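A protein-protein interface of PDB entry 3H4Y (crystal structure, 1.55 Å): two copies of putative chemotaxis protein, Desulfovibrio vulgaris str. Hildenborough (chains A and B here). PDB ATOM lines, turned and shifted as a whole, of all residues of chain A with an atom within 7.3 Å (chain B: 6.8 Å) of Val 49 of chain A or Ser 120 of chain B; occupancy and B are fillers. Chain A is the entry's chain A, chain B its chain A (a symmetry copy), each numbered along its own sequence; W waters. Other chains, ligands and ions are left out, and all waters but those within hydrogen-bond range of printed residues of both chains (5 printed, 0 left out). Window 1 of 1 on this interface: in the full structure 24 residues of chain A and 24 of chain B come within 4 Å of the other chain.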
ATOM      1  N   SER A  47      26.197 -11.273 -18.381  1.00  0.00           N
ATOM      2  CA  SER A  47      26.184 -12.328 -19.365  1.00  0.00           C
ATOM      3  C   SER A  47      27.588 -12.705 -19.753  1.00  0.00           C
ATOM      4  O   SER A  47      28.560 -11.939 -19.524  1.00  0.00           O
ATOM      5  CB  SER A  47      25.515 -11.858 -20.659  1.00  0.00           C
ATOM      6  OG  SER A  47      24.141 -11.505 -20.467  1.00  0.00           O
ATOM      7  N   ALA A  48      27.702 -13.877 -20.403  1.00  0.00           N
ATOM      8  CA  ALA A  48      28.896 -14.178 -21.139  1.00  0.00           C
ATOM      9  C   ALA A  48      28.544 -14.740 -22.507  1.00  0.00           C
ATOM     10  O   ALA A  48      27.589 -15.491 -22.633  1.00  0.00           O
ATOM     11  CB  ALA A  48      29.860 -15.178 -20.378  1.00  0.00           C
ATOM     12  N   VAL A  49      29.383 -14.423 -23.488  1.00  0.00           N
ATOM     13  CA  VAL A  49      29.185 -14.827 -24.892  1.00  0.00           C
ATOM     14  C   VAL A  49      30.439 -15.553 -25.350  1.00  0.00           C
ATOM     15  O   VAL A  49      31.539 -15.115 -25.048  1.00  0.00           O
ATOM     16  CB  VAL A  49      28.890 -13.609 -25.808  1.00  0.00           C
ATOM     17  CG1 VAL A  49      28.865 -13.998 -27.305  1.00  0.00           C
ATOM     18  CG2 VAL A  49      27.573 -12.912 -25.409  1.00  0.00           C
ATOM     19  N   ILE A  50      30.241 -16.675 -26.042  1.00  0.00           N
ATOM     20  CA  ILE A  50      31.302 -17.456 -26.681  1.00  0.00           C
ATOM     21  C   ILE A  50      30.909 -17.649 -28.125  1.00  0.00           C
ATOM     22  O   ILE A  50      29.773 -17.996 -28.441  1.00  0.00           O
ATOM     23  CB  ILE A  50      31.496 -18.810 -26.001  1.00  0.00           C
ATOM     24  CG1 ILE A  50      32.178 -18.585 -24.647  1.00  0.00           C
ATOM     25  CG2 ILE A  50      32.234 -19.825 -26.914  1.00  0.00           C
ATOM     26  CD1 ILE A  50      32.309 -19.821 -23.795  1.00  0.00           C
ATOM     27  N   GLY A  51      31.859 -17.451 -29.021  1.00  0.00           N
ATOM     28  CA  GLY A  51      31.655 -17.743 -30.444  1.00  0.00           C
ATOM     29  C   GLY A  51      32.070 -19.164 -30.732  1.00  0.00           C
ATOM     30  O   GLY A  51      33.080 -19.646 -30.201  1.00  0.00           O
ATOM     31  N   GLY A  58      28.349 -19.993 -35.044  1.00  0.00           N
ATOM     32  CA  GLY A  58      27.327 -19.396 -34.223  1.00  0.00           C
ATOM     33  C   GLY A  58      27.837 -18.953 -32.885  1.00  0.00           C
ATOM     34  O   GLY A  58      28.980 -18.525 -32.734  1.00  0.00           O
ATOM     35  N   SER A  59      26.954 -19.048 -31.890  1.00  0.00           N
ATOM     36  CA  SER A  59      27.213 -18.542 -30.559  1.00  0.00           C
ATOM     37  C   SER A  59      26.615 -19.390 -29.465  1.00  0.00           C
ATOM     38  O   SER A  59      25.630 -20.124 -29.660  1.00  0.00           O
ATOM     39  CB  SER A  59      26.591 -17.149 -30.425  1.00  0.00           C
ATOM     40  OG  SER A  59      26.993 -16.297 -31.468  1.00  0.00           O
ATOM     41  N   ILE A  60      27.228 -19.262 -28.281  1.00  0.00           N
ATOM     42  CA  ILE A  60      26.653 -19.790 -27.033  1.00  0.00           C
ATOM     43  C   ILE A  60      26.672 -18.601 -26.087  1.00  0.00           C
ATOM     44  O   ILE A  60      27.680 -17.893 -25.981  1.00  0.00           O
ATOM     45  CB  ILE A  60      27.482 -20.942 -26.462  1.00  0.00           C
ATOM     46  CG1 ILE A  60      27.417 -22.180 -27.352  1.00  0.00           C
ATOM     47  CG2 ILE A  60      27.013 -21.256 -24.995  1.00  0.00           C
ATOM     48  CD1 ILE A  60      28.378 -23.363 -26.941  1.00  0.00           C
ATOM     49  N   SER A  61      25.591 -18.377 -25.337  1.00  0.00           N
ATOM     50  CA  SER A  61      25.626 -17.334 -24.328  1.00  0.00           C
ATOM     51  C   SER A  61      24.845 -17.782 -23.081  1.00  0.00           C
ATOM     52  O   SER A  61      23.988 -18.652 -23.151  1.00  0.00           O
ATOM     53  CB  SER A  61      25.055 -16.022 -24.854  1.00  0.00           C
ATOM     54  OG  SER A  61      23.716 -16.152 -25.262  1.00  0.00           O
ATOM     55  N   VAL A  62      25.172 -17.153 -21.948  1.00  0.00           N
ATOM     56  CA  VAL A  62      24.464 -17.344 -20.680  1.00  0.00           C
ATOM     57  C   VAL A  62      24.240 -15.945 -20.099  1.00  0.00           C
ATOM     58  O   VAL A  62      25.194 -15.164 -19.997  1.00  0.00           O
ATOM     59  CB  VAL A  62      25.268 -18.204 -19.689  1.00  0.00           C
ATOM     60  CG1 VAL A  62      24.371 -18.611 -18.480  1.00  0.00           C
ATOM     61  CG2 VAL A  62      25.760 -19.469 -20.376  1.00  0.00           C
ATOM     62  N   THR A  63      22.999 -15.635 -19.736  1.00  0.00           N
ATOM     63  CA  THR A  63      22.591 -14.327 -19.231  1.00  0.00           C
ATOM     64  C   THR A  63      21.892 -14.521 -17.892  1.00  0.00           C
ATOM     65  O   THR A  63      20.881 -15.215 -17.795  1.00  0.00           O
ATOM     66  CB  THR A  63      21.642 -13.643 -20.227  1.00  0.00           C
ATOM     67  OG1 THR A  63      22.359 -13.430 -21.462  1.00  0.00           O
ATOM     68  CG2 THR A  63      21.065 -12.347 -19.668  1.00  0.00           C
ATOM     69  N   VAL A  92      31.516 -16.010 -14.023  1.00  0.00           N
ATOM     70  CA  VAL A  92      30.570 -16.115 -15.128  1.00  0.00           C
ATOM     71  C   VAL A  92      31.317 -16.577 -16.374  1.00  0.00           C
ATOM     72  O   VAL A  92      30.816 -17.416 -17.093  1.00  0.00           O
ATOM     73  CB  VAL A  92      29.745 -14.818 -15.370  1.00  0.00           C
ATOM     74  CG1 VAL A  92      28.907 -14.905 -16.590  1.00  0.00           C
ATOM     75  CG2 VAL A  92      28.828 -14.583 -14.138  1.00  0.00           C
ATOM     76  N   GLY A  93      32.494 -16.016 -16.635  1.00  0.00           N
ATOM     77  CA  GLY A  93      33.288 -16.464 -17.786  1.00  0.00           C
ATOM     78  C   GLY A  93      33.643 -17.955 -17.707  1.00  0.00           C
ATOM     79  O   GLY A  93      33.493 -18.685 -18.691  1.00  0.00           O
ATOM     80  N   THR A  96      30.587 -20.234 -18.151  1.00  0.00           N
ATOM     81  CA  THR A  96      30.206 -20.232 -19.559  1.00  0.00           C
ATOM     82  C   THR A  96      31.176 -21.028 -20.401  1.00  0.00           C
ATOM     83  O   THR A  96      30.765 -21.782 -21.283  1.00  0.00           O
ATOM     84  CB  THR A  96      30.000 -18.806 -20.079  1.00  0.00           C
ATOM     85  OG1 THR A  96      29.011 -18.186 -19.238  1.00  0.00           O
ATOM     86  CG2 THR A  96      29.492 -18.819 -21.513  1.00  0.00           C
ATOM     87  N   SER A 117      35.490 -20.244 -28.730  1.00  0.00           N
ATOM     88  CA  SER A 117      36.361 -19.152 -28.339  1.00  0.00           C
ATOM     89  C   SER A 117      36.435 -19.039 -26.798  1.00  0.00           C
ATOM     90  O   SER A 117      35.725 -19.710 -26.045  1.00  0.00           O
ATOM     91  CB  SER A 117      35.814 -17.839 -28.933  1.00  0.00           C
ATOM     92  OG  SER A 117      34.682 -17.369 -28.211  1.00  0.00           O
ATOM     93  N   THR A 118      37.263 -18.116 -26.340  1.00  0.00           N
ATOM     94  CA  THR A 118      37.208 -17.721 -24.940  1.00  0.00           C
ATOM     95  C   THR A 118      35.983 -16.798 -24.753  1.00  0.00           C
ATOM     96  O   THR A 118      35.388 -16.274 -25.694  1.00  0.00           O
ATOM     97  CB  THR A 118      38.497 -17.027 -24.508  1.00  0.00           C
ATOM     98  OG1 THR A 118      38.797 -15.967 -25.405  1.00  0.00           O
ATOM     99  CG2 THR A 118      39.651 -18.042 -24.502  1.00  0.00           C
ATOM    100  N   PRO A 119      35.517 -16.693 -23.509  1.00  0.00           N
ATOM    101  CA  PRO A 119      34.315 -15.897 -23.256  1.00  0.00           C
ATOM    102  C   PRO A 119      34.526 -14.393 -23.145  1.00  0.00           C
ATOM    103  O   PRO A 119      35.610 -13.929 -22.819  1.00  0.00           O
ATOM    104  CB  PRO A 119      33.825 -16.424 -21.907  1.00  0.00           C
ATOM    105  CG  PRO A 119      35.000 -17.007 -21.260  1.00  0.00           C
ATOM    106  CD  PRO A 119      36.055 -17.327 -22.295  1.00  0.00           C
ATOM    107  N   SER A 120      33.471 -13.650 -23.438  1.00  0.00           N
ATOM    108  CA  SER A 120      33.431 -12.192 -23.221  1.00  0.00           C
ATOM    109  C   SER A 120      32.294 -11.941 -22.252  1.00  0.00           C
ATOM    110  O   SER A 120      31.156 -12.351 -22.514  1.00  0.00           O
ATOM    111  CB  SER A 120      33.176 -11.456 -24.530  1.00  0.00           C
ATOM    112  OG  SER A 120      34.144 -11.863 -25.516  1.00  0.00           O
ATOM    113  N   VAL A 121      32.614 -11.293 -21.142  1.00  0.00           N
ATOM    114  CA  VAL A 121      31.639 -10.990 -20.099  1.00  0.00           C
ATOM    115  C   VAL A 121      31.071  -9.584 -20.294  1.00  0.00           C
ATOM    116  O   VAL A 121      31.797  -8.617 -20.491  1.00  0.00           O
ATOM    117  CB  VAL A 121      32.268 -11.167 -18.697  1.00  0.00           C
ATOM    118  CG1 VAL A 121      31.354 -10.619 -17.625  1.00  0.00           C
ATOM    119  CG2 VAL A 121      32.545 -12.670 -18.447  1.00  0.00           C
ATOM    120  N   ILE A 122      29.754  -9.522 -20.198  1.00  0.00           N
ATOM    121  CA  ILE A 122      29.000  -8.289 -20.349  1.00  0.00           C
ATOM    122  C   ILE A 122      28.352  -7.935 -19.042  1.00  0.00           C
ATOM    123  O   ILE A 122      27.701  -8.781 -18.400  1.00  0.00           O
ATOM    124  CB  ILE A 122      27.894  -8.403 -21.400  1.00  0.00           C
ATOM    125  CG1 ILE A 122      28.501  -8.673 -22.772  1.00  0.00           C
ATOM    126  CG2 ILE A 122      27.046  -7.125 -21.439  1.00  0.00           C
ATOM    127  CD1 ILE A 122      28.526 -10.178 -23.151  1.00  0.00           C
ATOM    128  N   THR A 128      20.879  -6.251 -23.121  1.00  0.00           N
ATOM    129  CA  THR A 128      20.385  -7.315 -23.995  1.00  0.00           C
ATOM    130  C   THR A 128      21.492  -7.931 -24.827  1.00  0.00           C
ATOM    131  O   THR A 128      22.485  -7.264 -25.172  1.00  0.00           O
ATOM    132  CB  THR A 128      19.277  -6.791 -24.933  1.00  0.00           C
ATOM    133  OG1 THR A 128      19.787  -5.728 -25.758  1.00  0.00           O
ATOM    134  CG2 THR A 128      18.045  -6.302 -24.093  1.00  0.00           C
ATOM    135  N   ILE A 129      21.316  -9.218 -25.097  1.00  0.00           N
ATOM    136  CA  ILE A 129      22.193 -10.007 -25.958  1.00  0.00           C
ATOM    137  C   ILE A 129      21.379 -10.436 -27.156  1.00  0.00           C
ATOM    138  O   ILE A 129      20.380 -11.160 -27.002  1.00  0.00           O
ATOM    139  CB  ILE A 129      22.707 -11.287 -25.255  1.00  0.00           C
ATOM    140  CG1 ILE A 129      23.384 -11.018 -23.911  1.00  0.00           C
ATOM    141  CG2 ILE A 129      23.639 -12.071 -26.211  1.00  0.00           C
ATOM    142  CD1 ILE A 129      24.624 -10.057 -23.999  1.00  0.00           C
ATOM    143  N   SER A 130      21.834 -10.051 -28.352  1.00  0.00           N
ATOM    144  CA  SER A 130      21.109 -10.355 -29.582  1.00  0.00           C
ATOM    145  C   SER A 130      22.064 -11.003 -30.562  1.00  0.00           C
ATOM    146  O   SER A 130      22.832 -10.329 -31.234  1.00  0.00           O
ATOM    147  CB  SER A 130      20.499  -9.092 -30.200  1.00  0.00           C
ATOM    148  OG  SER A 130      19.607  -8.468 -29.301  1.00  0.00           O
ATOM    149  N   HIS A 131      22.038 -12.323 -30.626  1.00  0.00           N
ATOM    150  CA  HIS A 131      22.822 -12.981 -31.659  1.00  0.00           C
ATOM    151  C   HIS A 131      22.255 -12.641 -33.044  1.00  0.00           C
ATOM    152  O   HIS A 131      21.041 -12.614 -33.258  1.00  0.00           O
ATOM    153  CB  HIS A 131      22.895 -14.491 -31.440  1.00  0.00           C
ATOM    154  CG  HIS A 131      23.326 -14.863 -30.068  1.00  0.00           C
ATOM    155  ND1 HIS A 131      24.527 -14.451 -29.539  1.00  0.00           N
ATOM    156  CD2 HIS A 131      22.685 -15.538 -29.086  1.00  0.00           C
ATOM    157  CE1 HIS A 131      24.624 -14.901 -28.299  1.00  0.00           C
ATOM    158  NE2 HIS A 131      23.518 -15.574 -28.003  1.00  0.00           N
ATOM    159  N   VAL A 132      23.159 -12.304 -33.958  1.00  0.00           N
ATOM    160  CA  VAL A 132      22.837 -11.873 -35.319  1.00  0.00           C
ATOM    161  C   VAL A 132      23.177 -13.046 -36.224  1.00  0.00           C
ATOM    162  O   VAL A 132      24.355 -13.354 -36.502  1.00  0.00           O
ATOM    163  CB  VAL A 132      23.655 -10.592 -35.693  1.00  0.00           C
ATOM    164  CG1 VAL A 132      23.450 -10.193 -37.181  1.00  0.00           C
ATOM    165  CG2 VAL A 132      23.271  -9.433 -34.782  1.00  0.00           C
ATOM    166  N   CYS A 154      23.035 -20.838 -31.069  1.00  0.00           N
ATOM    167  CA  CYS A 154      22.590 -20.769 -32.463  1.00  0.00           C
ATOM    168  C   CYS A 154      23.731 -21.137 -33.372  1.00  0.00           C
ATOM    169  O   CYS A 154      24.907 -21.075 -32.981  1.00  0.00           O
ATOM    170  CB  CYS A 154      22.098 -19.365 -32.801  1.00  0.00           C
ATOM    171  SG  CYS A 154      23.350 -18.046 -32.669  1.00  0.00           S
ATOM    172  N   SER B  47      27.484  -2.695 -28.624  1.00  0.00           N
ATOM    173  CA  SER B  47      28.676  -3.423 -28.984  1.00  0.00           C
ATOM    174  C   SER B  47      28.325  -4.639 -29.799  1.00  0.00           C
ATOM    175  O   SER B  47      27.158  -5.110 -29.805  1.00  0.00           O
ATOM    176  CB  SER B  47      29.387  -3.957 -27.738  1.00  0.00           C
ATOM    177  OG  SER B  47      29.834  -2.908 -26.873  1.00  0.00           O
ATOM    178  N   ALA B  48      29.357  -5.199 -30.456  1.00  0.00           N
ATOM    179  CA  ALA B  48      29.248  -6.539 -30.957  1.00  0.00           C
ATOM    180  C   ALA B  48      30.497  -7.334 -30.612  1.00  0.00           C
ATOM    181  O   ALA B  48      31.593  -6.797 -30.648  1.00  0.00           O
ATOM    182  CB  ALA B  48      28.984  -6.599 -32.518  1.00  0.00           C
ATOM    183  N   VAL B  49      30.302  -8.626 -30.367  1.00  0.00           N
ATOM    184  CA  VAL B  49      31.378  -9.549 -29.965  1.00  0.00           C
ATOM    185  C   VAL B  49      31.377 -10.719 -30.937  1.00  0.00           C
ATOM    186  O   VAL B  49      30.317 -11.217 -31.284  1.00  0.00           O
ATOM    187  CB  VAL B  49      31.197 -10.048 -28.506  1.00  0.00           C
ATOM    188  CG1 VAL B  49      32.212 -11.156 -28.138  1.00  0.00           C
ATOM    189  CG2 VAL B  49      31.282  -8.882 -27.500  1.00  0.00           C
ATOM    190  N   ILE B  50      32.573 -11.105 -31.382  1.00  0.00           N
ATOM    191  CA  ILE B  50      32.806 -12.283 -32.221  1.00  0.00           C
ATOM    192  C   ILE B  50      33.873 -13.108 -31.546  1.00  0.00           C
ATOM    193  O   ILE B  50      34.900 -12.596 -31.106  1.00  0.00           O
ATOM    194  CB  ILE B  50      33.251 -11.895 -33.630  1.00  0.00           C
ATOM    195  CG1 ILE B  50      32.044 -11.327 -34.385  1.00  0.00           C
ATOM    196  CG2 ILE B  50      33.957 -13.065 -34.365  1.00  0.00           C
ATOM    197  CD1 ILE B  50      32.362 -10.768 -35.749  1.00  0.00           C
ATOM    198  N   GLY B  51      33.652 -14.409 -31.481  1.00  0.00           N
ATOM    199  CA  GLY B  51      34.668 -15.344 -30.984  1.00  0.00           C
ATOM    200  C   GLY B  51      35.513 -15.829 -32.135  1.00  0.00           C
ATOM    201  O   GLY B  51      34.997 -16.094 -33.229  1.00  0.00           O
ATOM    202  N   SER B  59      38.899 -13.328 -29.003  1.00  0.00           N
ATOM    203  CA  SER B  59      37.758 -12.500 -29.326  1.00  0.00           C
ATOM    204  C   SER B  59      38.109 -11.281 -30.140  1.00  0.00           C
ATOM    205  O   SER B  59      39.246 -10.776 -30.118  1.00  0.00           O
ATOM    206  CB  SER B  59      37.123 -11.994 -28.027  1.00  0.00           C
ATOM    207  OG  SER B  59      36.853 -13.046 -27.135  1.00  0.00           O
ATOM    208  N   GLY B  93      26.189  -5.517 -36.077  1.00  0.00           N
ATOM    209  CA  GLY B  93      26.609  -6.905 -36.311  1.00  0.00           C
ATOM    210  C   GLY B  93      27.352  -7.075 -37.643  1.00  0.00           C
ATOM    211  O   GLY B  93      28.407  -7.714 -37.692  1.00  0.00           O
ATOM    212  N   THR B  96      30.799  -5.387 -37.645  1.00  0.00           N
ATOM    213  CA  THR B  96      31.713  -6.195 -36.845  1.00  0.00           C
ATOM    214  C   THR B  96      32.109  -7.465 -37.562  1.00  0.00           C
ATOM    215  O   THR B  96      33.276  -7.855 -37.543  1.00  0.00           O
ATOM    216  CB  THR B  96      31.148  -6.455 -35.445  1.00  0.00           C
ATOM    217  OG1 THR B  96      30.879  -5.172 -34.851  1.00  0.00           O
ATOM    218  CG2 THR B  96      32.156  -7.199 -34.582  1.00  0.00           C
ATOM    219  N   SER B 117      33.300 -16.575 -35.513  1.00  0.00           N
ATOM    220  CA  SER B 117      31.894 -16.858 -35.295  1.00  0.00           C
ATOM    221  C   SER B 117      31.012 -15.748 -35.913  1.00  0.00           C
ATOM    222  O   SER B 117      31.480 -14.712 -36.390  1.00  0.00           O
ATOM    223  CB  SER B 117      31.632 -16.949 -33.778  1.00  0.00           C
ATOM    224  OG  SER B 117      31.602 -15.661 -33.174  1.00  0.00           O
ATOM    225  N   THR B 118      29.708 -15.953 -35.829  1.00  0.00           N
ATOM    226  CA  THR B 118      28.783 -14.865 -36.110  1.00  0.00           C
ATOM    227  C   THR B 118      28.772 -13.919 -34.888  1.00  0.00           C
ATOM    228  O   THR B 118      29.231 -14.236 -33.791  1.00  0.00           O
ATOM    229  CB  THR B 118      27.383 -15.392 -36.416  1.00  0.00           C
ATOM    230  OG1 THR B 118      26.961 -16.268 -35.380  1.00  0.00           O
ATOM    231  CG2 THR B 118      27.398 -16.145 -37.756  1.00  0.00           C
ATOM    232  N   PRO B 119      28.348 -12.677 -35.115  1.00  0.00           N
ATOM    233  CA  PRO B 119      28.376 -11.697 -34.028  1.00  0.00           C
ATOM    234  C   PRO B 119      27.210 -11.757 -33.050  1.00  0.00           C
ATOM    235  O   PRO B 119      26.130 -12.228 -33.382  1.00  0.00           O
ATOM    236  CB  PRO B 119      28.328 -10.359 -34.764  1.00  0.00           C
ATOM    237  CG  PRO B 119      27.728 -10.644 -36.067  1.00  0.00           C
ATOM    238  CD  PRO B 119      27.858 -12.116 -36.385  1.00  0.00           C
ATOM    239  N   SER B 120      27.461 -11.285 -31.840  1.00  0.00           N
ATOM    240  CA  SER B 120      26.415 -11.100 -30.818  1.00  0.00           C
ATOM    241  C   SER B 120      26.409  -9.623 -30.482  1.00  0.00           C
ATOM    242  O   SER B 120      27.452  -9.069 -30.112  1.00  0.00           O
ATOM    243  CB  SER B 120      26.725 -11.919 -29.571  1.00  0.00           C
ATOM    244  OG  SER B 120      26.937 -13.296 -29.932  1.00  0.00           O
ATOM    245  N   VAL B 121      25.250  -9.000 -30.635  1.00  0.00           N
ATOM    246  CA  VAL B 121      25.082  -7.575 -30.374  1.00  0.00           C
ATOM    247  C   VAL B 121      24.572  -7.352 -28.949  1.00  0.00           C
ATOM    248  O   VAL B 121      23.623  -7.981 -28.498  1.00  0.00           O
ATOM    249  CB  VAL B 121      24.146  -6.935 -31.426  1.00  0.00           C
ATOM    250  CG1 VAL B 121      23.768  -5.527 -31.023  1.00  0.00           C
ATOM    251  CG2 VAL B 121      24.856  -6.924 -32.802  1.00  0.00           C
ATOM    252  N   ILE B 122      25.226  -6.411 -28.290  1.00  0.00           N
ATOM    253  CA  ILE B 122      24.914  -6.032 -26.922  1.00  0.00           C
ATOM    254  C   ILE B 122      24.397  -4.623 -26.898  1.00  0.00           C
ATOM    255  O   ILE B 122      25.003  -3.708 -27.489  1.00  0.00           O
ATOM    256  CB  ILE B 122      26.136  -6.093 -26.003  1.00  0.00           C
ATOM    257  CG1 ILE B 122      26.654  -7.524 -25.914  1.00  0.00           C
ATOM    258  CG2 ILE B 122      25.792  -5.567 -24.604  1.00  0.00           C
ATOM    259  CD1 ILE B 122      27.820  -7.820 -26.895  1.00  0.00           C
HETATM  260  O   HOH W   1      25.674 -15.056 -33.444  1.00  0.00           O
HETATM  261  O   HOH W   2      37.762 -13.667 -24.691  1.00  0.00           O
HETATM  262  O   HOH W   3      21.108  -6.632 -27.970  1.00  0.00           O
HETATM  263  O   HOH W   4      29.067 -14.618 -30.931  1.00  0.00           O
HETATM  264  O   HOH W   5      34.310 -14.014 -27.136  1.00  0.00           O
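The side-chain hydroxyl (OG) of Ser 120 of chain B is in hydrogen-bond range of the side-chain hydroxyl (OG) of Ser 59 of chain A, 3.4 Å away. OG of Ser 120 of chain A is in hydrogen-bond range of OG of Ser 59 of chain B (3.4 Å). The backbone NH of Ser 130 of chain A lies within hydrogen-bond range of the backbone carbonyl oxygen of Val 121 of chain B, at 2.7 Å. ND1 of His 131 of chain A is in hydrogen-bond range of OG of Ser 120 of chain B (2.7 Å). N of Val 132 of chain A sits at hydrogen-bond distance from O of Pro 119 of chain B, 3.0 Å away.
O of Ser 120 of chain A sits at hydrogen-bond distance from N of Val 49 of chain A, at 2.9 Å. N of Ser 117 of chain A is in hydrogen-bond range of O of Gly 51 of chain A. The backbone carbonyl oxygen (O) of Ser 59 of chain A sits at hydrogen-bond distance from the backbone NH (N) of Cys 154 of chain A, 3.0 Å away. The side-chain hydroxyl (OG) of Ser 61 of chain A is in hydrogen-bond range of a ring nitrogen (NE2) of His 131 of chain A, 2.8 Å away. N of Ile 122 of chain B lies within hydrogen-bond range of O of Ser 47 of chain B, 2.8 Å away. The backbone NH of Val 49 of chain B is in hydrogen-bond range of the backbone carbonyl oxygen of Ser 120 of chain B (2.9 Å).
Among the printed residues, merely in contact across the chains: Thr 128 of chain A with Ile 122 of chain B, Gly 58 of chain A with Ser 117 of chain B, Ser 120 of chain A with Val 49 of chain B, Val 49 of chain A with Ser 120 of chain B, Gly 58 of chain A with Thr 118 of chain B, Ser 117 of chain A with Gly 51 of chain B, Gly 51 of chain A with Ser 117 of chain B, Ile 129 of chain A with Val 121 of chain B, Val 132 of chain A with Val 121 of chain B, Thr 128 of chain A with Val 121 of chain B, Val 132 of chain A with Thr 118 of chain B, Ser 130 of chain A with Ser 120 of chain B, Ile 122 of chain A with Ile 122 of chain B, Ile 129 of chain A with Ile 122 of chain B, His 131 of chain A with Pro 119 of chain B, Thr 118 of chain A with Ser 59 of chain B, Ser 59 of chain A with Thr 118 of chain B and Gly 51 of chain A with Gly 51 of chain B.
Of the printed residues of chain B, Val 49 of chain A touches Ser 120. Of the printed residues of chain A, Ser 120 of chain B touches Val 49, Ser 59, Ser 130 and His 131. Printed residues of chain B within 4 Å of His 131 of chain A: Pro 119 and Ser 120. Of the printed residues of chain A, Thr 118 of chain B touches Gly 58 (3.4 Å), Ser 59 (3.8 Å) and Val 132 (3.7 Å). Printed residues of chain A within 4 Å of Ser 59 of chain B: Thr 118 (3.8 Å) and Ser 120 (3.4 Å). Of the printed residues of chain B, Ser 117 of chain A touches Gly 51. The nearest printed residue of chain B that does not touch Val 49 of chain A is Val 49 of chain B (4.5 Å).
Of the 14 printed residues of chain B, 9 touch a printed residue of chain A. Printed residues of chain B that touch a printed residue of chain A: Val 49, Gly 51, Ser 59, Ser 117, Thr 118, Pro 119, Ser 120, Val 121 and Ile 122. Hydrophobic or aromatic side chains of chain B that line the printed part of chain A: Val 49, Pro 119, Val 121 and Ile 122. Printed residues of chain A that touch a printed residue of chain B: Val 49, Gly 51, Gly 58, Ser 59, Ser 117, Thr 118, Ser 120, Ile 122, Thr 128, Ile 129, Ser 130, His 131 and Val 132. Hydrophobic or aromatic side chains of chain A that line the printed part of chain B: Val 49, Ile 122, Ile 129, His 131 and Val 132. Among the printed residues, 23 pairs touch across the chains.
Val 49 of chain A touches Ser 120 of chain B, and with the chains exchanged Ser 120 of chain A touches Val 49 of chain B. Gly 51 of chain A touches its own counterpart, Gly 51 of chain B. Ser 59 of chain A touches Ser 120 of chain B, and with the chains exchanged Ser 120 of chain A touches Ser 59 of chain B. Ile 122 of chain B touches its own counterpart, Ile 122 of chain A. Positions printed for both chains: 47, 48, 49, 50, 51, 59, 93, 96, 117, 118, 119, 120, 121 and 122. Of the 23 pairs that touch across the chains among the printed residues, 10 have their exchanged pair printed and touching as well.
Water W2 lies within hydrogen-bond range of OG1 of Thr 118 of chain A, OG of Ser 59 of chain B and O of Pro 119 of chain A. Water W1 lies within hydrogen-bond range of OG1 of Thr 118 of chain B, OG of Ser 59 of chain A and O of Pro 119 of chain B. Water W4 lies within hydrogen-bond range of the side-chain hydroxyl of Ser 120 of chain B (2.7 Å), the side-chain hydroxyl of Ser 59 of chain A (2.7 Å) and the backbone carbonyl oxygen of Thr 118 of chain B (2.9 Å). Water W5 lies within hydrogen-bond range of OG of Ser 120 of chain A (2.7 Å), OG of Ser 59 of chain B (2.7 Å) and O of Thr 118 of chain A (2.9 Å). Water W3 lies within hydrogen-bond range of the side-chain hydroxyl of Ser 130 of chain A, the side-chain hydroxyl of Thr 128 of chain A and the backbone carbonyl oxygen of Val 121 of chain B.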
